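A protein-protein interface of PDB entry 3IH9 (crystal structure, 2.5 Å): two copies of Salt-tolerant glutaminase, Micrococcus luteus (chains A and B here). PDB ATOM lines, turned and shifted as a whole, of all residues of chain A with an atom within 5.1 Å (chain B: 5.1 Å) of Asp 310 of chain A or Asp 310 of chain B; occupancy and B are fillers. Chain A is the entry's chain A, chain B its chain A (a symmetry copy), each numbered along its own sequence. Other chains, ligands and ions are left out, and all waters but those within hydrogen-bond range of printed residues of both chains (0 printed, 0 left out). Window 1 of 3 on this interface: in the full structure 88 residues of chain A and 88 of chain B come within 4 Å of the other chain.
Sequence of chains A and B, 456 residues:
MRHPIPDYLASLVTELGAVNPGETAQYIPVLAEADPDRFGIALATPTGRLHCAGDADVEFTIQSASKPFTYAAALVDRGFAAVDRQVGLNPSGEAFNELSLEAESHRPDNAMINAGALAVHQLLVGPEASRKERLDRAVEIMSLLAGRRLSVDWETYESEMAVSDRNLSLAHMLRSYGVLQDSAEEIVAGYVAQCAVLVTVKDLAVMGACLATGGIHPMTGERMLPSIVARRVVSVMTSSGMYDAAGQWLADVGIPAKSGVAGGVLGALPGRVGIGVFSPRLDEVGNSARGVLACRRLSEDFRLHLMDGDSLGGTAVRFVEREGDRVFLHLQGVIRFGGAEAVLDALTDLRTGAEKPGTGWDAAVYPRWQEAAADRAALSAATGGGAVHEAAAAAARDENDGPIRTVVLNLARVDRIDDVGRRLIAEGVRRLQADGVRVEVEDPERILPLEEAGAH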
ATOM      1  N   GLY A 271      -3.732 -17.308   6.539  1.00  0.00           N
ATOM      2  CA  GLY A 271      -4.898 -17.584   5.720  1.00  0.00           C
ATOM      3  C   GLY A 271      -5.354 -16.497   4.763  1.00  0.00           C
ATOM      4  O   GLY A 271      -6.364 -16.674   4.090  1.00  0.00           O
ATOM      5  N   ARG A 272      -4.629 -15.389   4.661  1.00  0.00           N
ATOM      6  CA  ARG A 272      -5.084 -14.329   3.773  1.00  0.00           C
ATOM      7  C   ARG A 272      -4.149 -13.722   2.741  1.00  0.00           C
ATOM      8  O   ARG A 272      -4.555 -13.545   1.604  1.00  0.00           O
ATOM      9  CB  ARG A 272      -5.727 -13.211   4.606  1.00  0.00           C
ATOM     10  CG  ARG A 272      -7.180 -13.510   4.951  1.00  0.00           C
ATOM     11  CD  ARG A 272      -7.700 -12.669   6.091  1.00  0.00           C
ATOM     12  NE  ARG A 272      -7.096 -13.052   7.359  1.00  0.00           N
ATOM     13  CZ  ARG A 272      -7.342 -12.440   8.511  1.00  0.00           C
ATOM     14  NH1 ARG A 272      -8.189 -11.419   8.548  1.00  0.00           N
ATOM     15  NH2 ARG A 272      -6.734 -12.842   9.621  1.00  0.00           N
ATOM     16  N   ASP A 308      -9.355  -9.754  12.909  1.00  0.00           N
ATOM     17  CA  ASP A 308     -10.633  -9.714  12.201  1.00  0.00           C
ATOM     18  C   ASP A 308     -10.869 -11.109  11.687  1.00  0.00           C
ATOM     19  O   ASP A 308     -10.352 -11.516  10.649  1.00  0.00           O
ATOM     20  CB  ASP A 308     -10.592  -8.714  11.051  1.00  0.00           C
ATOM     21  CG  ASP A 308     -10.926  -7.300  11.499  1.00  0.00           C
ATOM     22  OD1 ASP A 308     -10.429  -6.337  10.877  1.00  0.00           O
ATOM     23  OD2 ASP A 308     -11.697  -7.143  12.468  1.00  0.00           O
ATOM     24  N   GLY A 309     -11.667 -11.843  12.442  1.00  0.00           N
ATOM     25  CA  GLY A 309     -11.937 -13.222  12.085  1.00  0.00           C
ATOM     26  C   GLY A 309     -12.482 -13.488  10.698  1.00  0.00           C
ATOM     27  O   GLY A 309     -13.334 -12.776  10.170  1.00  0.00           O
ATOM     28  N   ASP A 310     -11.978 -14.570  10.134  1.00  0.00           N
ATOM     29  CA  ASP A 310     -12.406 -14.951   8.814  1.00  0.00           C
ATOM     30  C   ASP A 310     -12.280 -16.466   8.703  1.00  0.00           C
ATOM     31  O   ASP A 310     -11.290 -16.975   8.189  1.00  0.00           O
ATOM     32  CB  ASP A 310     -11.530 -14.247   7.787  1.00  0.00           C
ATOM     33  CG  ASP A 310     -11.982 -14.495   6.379  1.00  0.00           C
ATOM     34  OD1 ASP A 310     -12.707 -15.494   6.176  1.00  0.00           O
ATOM     35  OD2 ASP A 310     -11.609 -13.707   5.477  1.00  0.00           O
ATOM     36  N   SER A 311     -13.294 -17.177   9.187  1.00  0.00           N
ATOM     37  CA  SER A 311     -13.290 -18.633   9.163  1.00  0.00           C
ATOM     38  C   SER A 311     -14.358 -19.246   8.283  1.00  0.00           C
ATOM     39  O   SER A 311     -15.326 -18.592   7.913  1.00  0.00           O
ATOM     40  CB  SER A 311     -13.462 -19.188  10.577  1.00  0.00           C
ATOM     41  OG  SER A 311     -12.373 -18.825  11.407  1.00  0.00           O
ATOM     42  N   LEU A 312     -14.163 -20.519   7.960  1.00  0.00           N
ATOM     43  CA  LEU A 312     -15.106 -21.288   7.153  1.00  0.00           C
ATOM     44  C   LEU A 312     -16.374 -21.522   7.989  1.00  0.00           C
ATOM     45  O   LEU A 312     -17.493 -21.305   7.521  1.00  0.00           O
ATOM     46  CB  LEU A 312     -14.477 -22.634   6.774  1.00  0.00           C
ATOM     47  CG  LEU A 312     -15.326 -23.654   6.020  1.00  0.00           C
ATOM     48  CD1 LEU A 312     -15.606 -23.142   4.619  1.00  0.00           C
ATOM     49  CD2 LEU A 312     -14.587 -24.984   5.953  1.00  0.00           C
ATOM     50  N   VAL A 334     -11.570 -25.906   3.348  1.00  0.00           N
ATOM     51  CA  VAL A 334     -10.410 -26.417   4.071  1.00  0.00           C
ATOM     52  C   VAL A 334     -10.872 -26.716   5.498  1.00  0.00           C
ATOM     53  O   VAL A 334     -10.910 -25.826   6.346  1.00  0.00           O
ATOM     54  CB  VAL A 334      -9.265 -25.368   4.086  1.00  0.00           C
ATOM     55  CG1 VAL A 334      -8.102 -25.859   4.941  1.00  0.00           C
ATOM     56  CG2 VAL A 334      -8.794 -25.109   2.664  1.00  0.00           C
ATOM     57  N   ARG A 336     -10.807 -27.748   9.176  1.00  0.00           N
ATOM     58  CA  ARG A 336      -9.920 -27.799  10.328  1.00  0.00           C
ATOM     59  C   ARG A 336     -10.858 -27.816  11.526  1.00  0.00           C
ATOM     60  O   ARG A 336     -12.022 -28.171  11.380  1.00  0.00           O
ATOM     61  CB  ARG A 336      -9.018 -26.568  10.368  1.00  0.00           C
ATOM     62  CG  ARG A 336      -8.197 -26.394   9.115  1.00  0.00           C
ATOM     63  CD  ARG A 336      -7.332 -25.161   9.201  1.00  0.00           C
ATOM     64  NE  ARG A 336      -6.070 -25.406   9.888  1.00  0.00           N
ATOM     65  CZ  ARG A 336      -5.485 -24.520  10.688  1.00  0.00           C
ATOM     66  NH1 ARG A 336      -6.066 -23.347  10.899  1.00  0.00           N
ATOM     67  NH2 ARG A 336      -4.322 -24.798  11.261  1.00  0.00           N
ATOM     68  N   PHE A 337     -10.383 -27.433  12.701  1.00  0.00           N
ATOM     69  CA  PHE A 337     -11.255 -27.447  13.867  1.00  0.00           C
ATOM     70  C   PHE A 337     -12.589 -26.731  13.615  1.00  0.00           C
ATOM     71  O   PHE A 337     -13.663 -27.282  13.876  1.00  0.00           O
ATOM     72  CB  PHE A 337     -10.568 -26.808  15.075  1.00  0.00           C
ATOM     73  CG  PHE A 337     -11.419 -26.817  16.307  1.00  0.00           C
ATOM     74  CD1 PHE A 337     -11.556 -27.976  17.065  1.00  0.00           C
ATOM     75  CD2 PHE A 337     -12.147 -25.687  16.674  1.00  0.00           C
ATOM     76  CE1 PHE A 337     -12.410 -28.013  18.170  1.00  0.00           C
ATOM     77  CE2 PHE A 337     -13.004 -25.715  17.774  1.00  0.00           C
ATOM     78  CZ  PHE A 337     -13.135 -26.879  18.523  1.00  0.00           C
ATOM     79  N   GLY A 338     -12.519 -25.504  13.114  1.00  0.00           N
ATOM     80  CA  GLY A 338     -13.727 -24.743  12.849  1.00  0.00           C
ATOM     81  C   GLY A 338     -14.769 -25.496  12.045  1.00  0.00           C
ATOM     82  O   GLY A 338     -15.922 -25.610  12.463  1.00  0.00           O
ATOM     83  N   GLY A 339     -14.365 -26.005  10.884  1.00  0.00           N
ATOM     84  CA  GLY A 339     -15.278 -26.748  10.036  1.00  0.00           C
ATOM     85  C   GLY A 339     -15.666 -28.090  10.628  1.00  0.00           C
ATOM     86  O   GLY A 339     -16.828 -28.475  10.590  1.00  0.00           O
ATOM     87  N   GLY B 271     -13.058 -15.467  15.040  1.00  0.00           N
ATOM     88  CA  GLY B 271     -13.706 -16.396  14.131  1.00  0.00           C
ATOM     89  C   GLY B 271     -13.800 -17.848  14.564  1.00  0.00           C
ATOM     90  O   GLY B 271     -14.295 -18.672  13.802  1.00  0.00           O
ATOM     91  N   ARG B 272     -13.363 -18.185  15.772  1.00  0.00           N
ATOM     92  CA  ARG B 272     -13.417 -19.583  16.176  1.00  0.00           C
ATOM     93  C   ARG B 272     -14.050 -19.989  17.495  1.00  0.00           C
ATOM     94  O   ARG B 272     -14.812 -20.942  17.519  1.00  0.00           O
ATOM     95  CB  ARG B 272     -12.014 -20.195  16.068  1.00  0.00           C
ATOM     96  CG  ARG B 272     -11.686 -20.644  14.649  1.00  0.00           C
ATOM     97  CD  ARG B 272     -10.208 -20.849  14.422  1.00  0.00           C
ATOM     98  NE  ARG B 272      -9.486 -19.585  14.419  1.00  0.00           N
ATOM     99  CZ  ARG B 272      -8.169 -19.485  14.288  1.00  0.00           C
ATOM    100  NH1 ARG B 272      -7.435 -20.582  14.143  1.00  0.00           N
ATOM    101  NH2 ARG B 272      -7.585 -18.292  14.313  1.00  0.00           N
ATOM    102  N   ASP B 308      -2.782 -19.930  13.106  1.00  0.00           N
ATOM    103  CA  ASP B 308      -3.144 -21.060  12.251  1.00  0.00           C
ATOM    104  C   ASP B 308      -4.315 -20.598  11.424  1.00  0.00           C
ATOM    105  O   ASP B 308      -5.463 -20.612  11.859  1.00  0.00           O
ATOM    106  CB  ASP B 308      -3.518 -22.280  13.084  1.00  0.00           C
ATOM    107  CG  ASP B 308      -2.305 -23.111  13.474  1.00  0.00           C
ATOM    108  OD1 ASP B 308      -2.339 -23.766  14.536  1.00  0.00           O
ATOM    109  OD2 ASP B 308      -1.315 -23.122  12.712  1.00  0.00           O
ATOM    110  N   GLY B 309      -3.998 -20.184  10.210  1.00  0.00           N
ATOM    111  CA  GLY B 309      -5.027 -19.669   9.329  1.00  0.00           C
ATOM    112  C   GLY B 309      -6.221 -20.558   9.058  1.00  0.00           C
ATOM    113  O   GLY B 309      -6.120 -21.769   8.869  1.00  0.00           O
ATOM    114  N   ASP B 310      -7.366 -19.901   9.011  1.00  0.00           N
ATOM    115  CA  ASP B 310      -8.588 -20.617   8.758  1.00  0.00           C
ATOM    116  C   ASP B 310      -9.553 -19.659   8.069  1.00  0.00           C
ATOM    117  O   ASP B 310     -10.406 -19.059   8.713  1.00  0.00           O
ATOM    118  CB  ASP B 310      -9.153 -21.115  10.080  1.00  0.00           C
ATOM    119  CG  ASP B 310     -10.369 -21.974   9.899  1.00  0.00           C
ATOM    120  OD1 ASP B 310     -10.991 -21.869   8.819  1.00  0.00           O
ATOM    121  OD2 ASP B 310     -10.711 -22.741  10.831  1.00  0.00           O
ATOM    122  N   SER B 311      -9.412 -19.528   6.753  1.00  0.00           N
ATOM    123  CA  SER B 311     -10.256 -18.630   5.977  1.00  0.00           C
ATOM    124  C   SER B 311     -11.157 -19.325   4.980  1.00  0.00           C
ATOM    125  O   SER B 311     -10.943 -20.480   4.631  1.00  0.00           O
ATOM    126  CB  SER B 311      -9.397 -17.618   5.218  1.00  0.00           C
ATOM    127  OG  SER B 311      -8.680 -16.782   6.109  1.00  0.00           O
ATOM    128  N   LEU B 312     -12.167 -18.594   4.525  1.00  0.00           N
ATOM    129  CA  LEU B 312     -13.116 -19.082   3.529  1.00  0.00           C
ATOM    130  C   LEU B 312     -12.381 -19.201   2.184  1.00  0.00           C
ATOM    131  O   LEU B 312     -12.472 -20.222   1.499  1.00  0.00           O
ATOM    132  CB  LEU B 312     -14.279 -18.089   3.399  1.00  0.00           C
ATOM    133  CG  LEU B 312     -15.340 -18.340   2.331  1.00  0.00           C
ATOM    134  CD1 LEU B 312     -16.146 -19.572   2.698  1.00  0.00           C
ATOM    135  CD2 LEU B 312     -16.257 -17.128   2.229  1.00  0.00           C
ATOM    136  N   VAL B 334     -19.341 -16.249   4.771  1.00  0.00           N
ATOM    137  CA  VAL B 334     -19.216 -14.885   5.272  1.00  0.00           C
ATOM    138  C   VAL B 334     -18.159 -14.191   4.413  1.00  0.00           C
ATOM    139  O   VAL B 334     -16.962 -14.311   4.669  1.00  0.00           O
ATOM    140  CB  VAL B 334     -18.782 -14.885   6.763  1.00  0.00           C
ATOM    141  CG1 VAL B 334     -18.539 -13.460   7.249  1.00  0.00           C
ATOM    142  CG2 VAL B 334     -19.859 -15.546   7.607  1.00  0.00           C
ATOM    143  N   ARG B 336     -15.768 -11.527   3.076  1.00  0.00           N
ATOM    144  CA  ARG B 336     -14.994 -10.373   3.507  1.00  0.00           C
ATOM    145  C   ARG B 336     -13.892 -10.248   2.465  1.00  0.00           C
ATOM    146  O   ARG B 336     -14.038 -10.763   1.363  1.00  0.00           O
ATOM    147  CB  ARG B 336     -14.400 -10.610   4.893  1.00  0.00           C
ATOM    148  CG  ARG B 336     -15.441 -10.929   5.937  1.00  0.00           C
ATOM    149  CD  ARG B 336     -14.803 -11.164   7.284  1.00  0.00           C
ATOM    150  NE  ARG B 336     -14.571  -9.928   8.020  1.00  0.00           N
ATOM    151  CZ  ARG B 336     -13.509  -9.719   8.790  1.00  0.00           C
ATOM    152  NH1 ARG B 336     -12.588 -10.666   8.904  1.00  0.00           N
ATOM    153  NH2 ARG B 336     -13.374  -8.579   9.455  1.00  0.00           N
ATOM    154  N   PHE B 337     -12.793  -9.584   2.791  1.00  0.00           N
ATOM    155  CA  PHE B 337     -11.725  -9.440   1.812  1.00  0.00           C
ATOM    156  C   PHE B 337     -11.326 -10.778   1.172  1.00  0.00           C
ATOM    157  O   PHE B 337     -11.266 -10.900  -0.055  1.00  0.00           O
ATOM    158  CB  PHE B 337     -10.486  -8.800   2.439  1.00  0.00           C
ATOM    159  CG  PHE B 337      -9.365  -8.611   1.465  1.00  0.00           C
ATOM    160  CD1 PHE B 337      -9.385  -7.556   0.558  1.00  0.00           C
ATOM    161  CD2 PHE B 337      -8.320  -9.531   1.400  1.00  0.00           C
ATOM    162  CE1 PHE B 337      -8.382  -7.421  -0.405  1.00  0.00           C
ATOM    163  CE2 PHE B 337      -7.315  -9.405   0.440  1.00  0.00           C
ATOM    164  CZ  PHE B 337      -7.346  -8.348  -0.463  1.00  0.00           C
ATOM    165  N   GLY B 338     -11.049 -11.774   2.004  1.00  0.00           N
ATOM    166  CA  GLY B 338     -10.654 -13.075   1.494  1.00  0.00           C
ATOM    167  C   GLY B 338     -11.577 -13.627   0.425  1.00  0.00           C
ATOM    168  O   GLY B 338     -11.130 -13.982  -0.666  1.00  0.00           O
ATOM    169  N   GLY B 339     -12.867 -13.706   0.742  1.00  0.00           N
ATOM    170  CA  GLY B 339     -13.839 -14.216  -0.207  1.00  0.00           C
ATOM    171  C   GLY B 339     -14.059 -13.278  -1.379  1.00  0.00           C
ATOM    172  O   GLY B 339     -14.135 -13.715  -2.521  1.00  0.00           O
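Of the printed residues of chain B, Asp 310 of chain A touches Asp 310 (2.3 Å), Ser 311 (2.9 Å), Leu 312 (3.6 Å) and Arg 336 (3.9 Å).
Of the printed residues of chain A, Asp 310 of chain B touches Asp 310, Ser 311, Leu 312 and Arg 336.
Of the printed residues of chain A, Gly 271 of chain B touches Gly 309 and Ser 311.
Printed residues of chain A within 4 Å of Arg 336 of chain B: Asp 308 (3.0 Å), Gly 309 (2.6 Å) and Asp 310 (3.9 Å).
Of the printed residues of chain A, Asp 308 of chain B touches Arg 336 (3.0 Å).
Of the printed residues of chain B, Gly 271 of chain A touches Gly 309 (3.9 Å) and Ser 311 (3.1 Å).
Of the printed residues of chain A, Leu 312 of chain B touches Asp 310.
Gly 338 of chain B touches none of the printed residues of chain A.
The guanidinium group (NH1) of Arg 272 of chain B is in hydrogen-bond range of the backbone carbonyl oxygen (O) of Asp 308 of chain B (3.0 Å).
The guanidinium group (NH1) of Arg 272 of chain A lies within hydrogen-bond range of the backbone carbonyl oxygen (O) of Asp 308 of chain A, at 3.0 Å.
Gly 271 of chain A touches Gly 309 of chain B, and with the chains exchanged Gly 309 of chain A touches Gly 271 of chain B.
Asp 308 of chain A touches Arg 336 of chain B, and with the chains exchanged Arg 336 of chain A touches Asp 308 of chain B.
Asp 310 of chain A touches its own counterpart, Asp 310 of chain B.
Asp 310 of chain A touches Leu 312 of chain B, and with the chains exchanged Leu 312 of chain A touches Asp 310 of chain B.
Positions printed for both chains: 271, 272, 308, 309, 310, 311, 312, 334, 336, 337, 338 and 339.
Of the 17 pairs that touch across the chains among the printed residues, 17 have their exchanged pair printed and touching as well.
The side-chain hydroxyl (OG) of Ser 311 of chain B lies close to the backbone carbonyl oxygen (O) of Asp 310 of chain A, 3.3 Å away.
The backbone carbonyl oxygen of Asp 310 of chain A sits close to the backbone carbonyl oxygen of Asp 310 of chain B (2.3 Å).
OG of Ser 311 of chain A is in hydrogen-bond range of O of Gly 271 of chain B.
The guanidinium group (NH2) of Arg 336 of chain A lies within salt-bridge range of the side-chain carboxylate (OD2) of Asp 308 of chain B, 3.7 Å away.
NH1 of Arg 336 of chain B is in hydrogen-bond range of O of Gly 309 of chain A (2.6 Å).
The side-chain carboxylate (OD2) of Asp 308 of chain A lies within salt-bridge range of the guanidinium group (NH2) of Arg 336 of chain B (3.7 Å).
The backbone carbonyl oxygen of Gly 309 of chain B sits at hydrogen-bond distance from the guanidinium group of Arg 336 of chain A, at 2.6 Å.
The side-chain hydroxyl (OG) of Ser 311 of chain A lies close to the backbone carbonyl oxygen (O) of Asp 310 of chain B (3.3 Å).
OG of Ser 311 of chain B sits at hydrogen-bond distance from O of Gly 271 of chain A (3.1 Å).
Printed residues of chain B that touch a printed residue of chain A: Gly 271, Arg 272, Asp 308, Gly 309, Asp 310, Ser 311, Leu 312 and Arg 336.
Of the 12 printed residues of chain A, 8 touch a printed residue of chain B.
Printed residues of chain A that touch a printed residue of chain B: Gly 271, Arg 272, Asp 308, Gly 309, Asp 310, Ser 311, Leu 312 and Arg 336.
Among the printed residues, Asp or Glu carboxylates within 4 Å of a Lys or Arg side-chain nitrogen of the other chain: Asp 308 of chain A with Arg 336 of chain B and Arg 336 of chain A with Asp 308 of chain B.
Gly 271 of chain A touches Gly 309 of chain B.
Arg 272 of chain A touches Ser 311 of chain B (CG to OG, 3.8 Å).
Gly 309 of chain A touches Gly 271 of chain B (CA to N, 3.9 Å).
OD1 of Asp 310 of chain A touches N of Leu 312 of chain B (3.6 Å).
NH1 of Arg 336 of chain B touches CB of Asp 310 of chain A, 3.9 Å away.
OG of Ser 311 of chain A touches CG of Arg 272 of chain B, at 3.8 Å.
N of Leu 312 of chain A touches OD1 of Asp 310 of chain B, 3.6 Å away.
Arg 336 of chain A touches Asp 310 of chain B.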
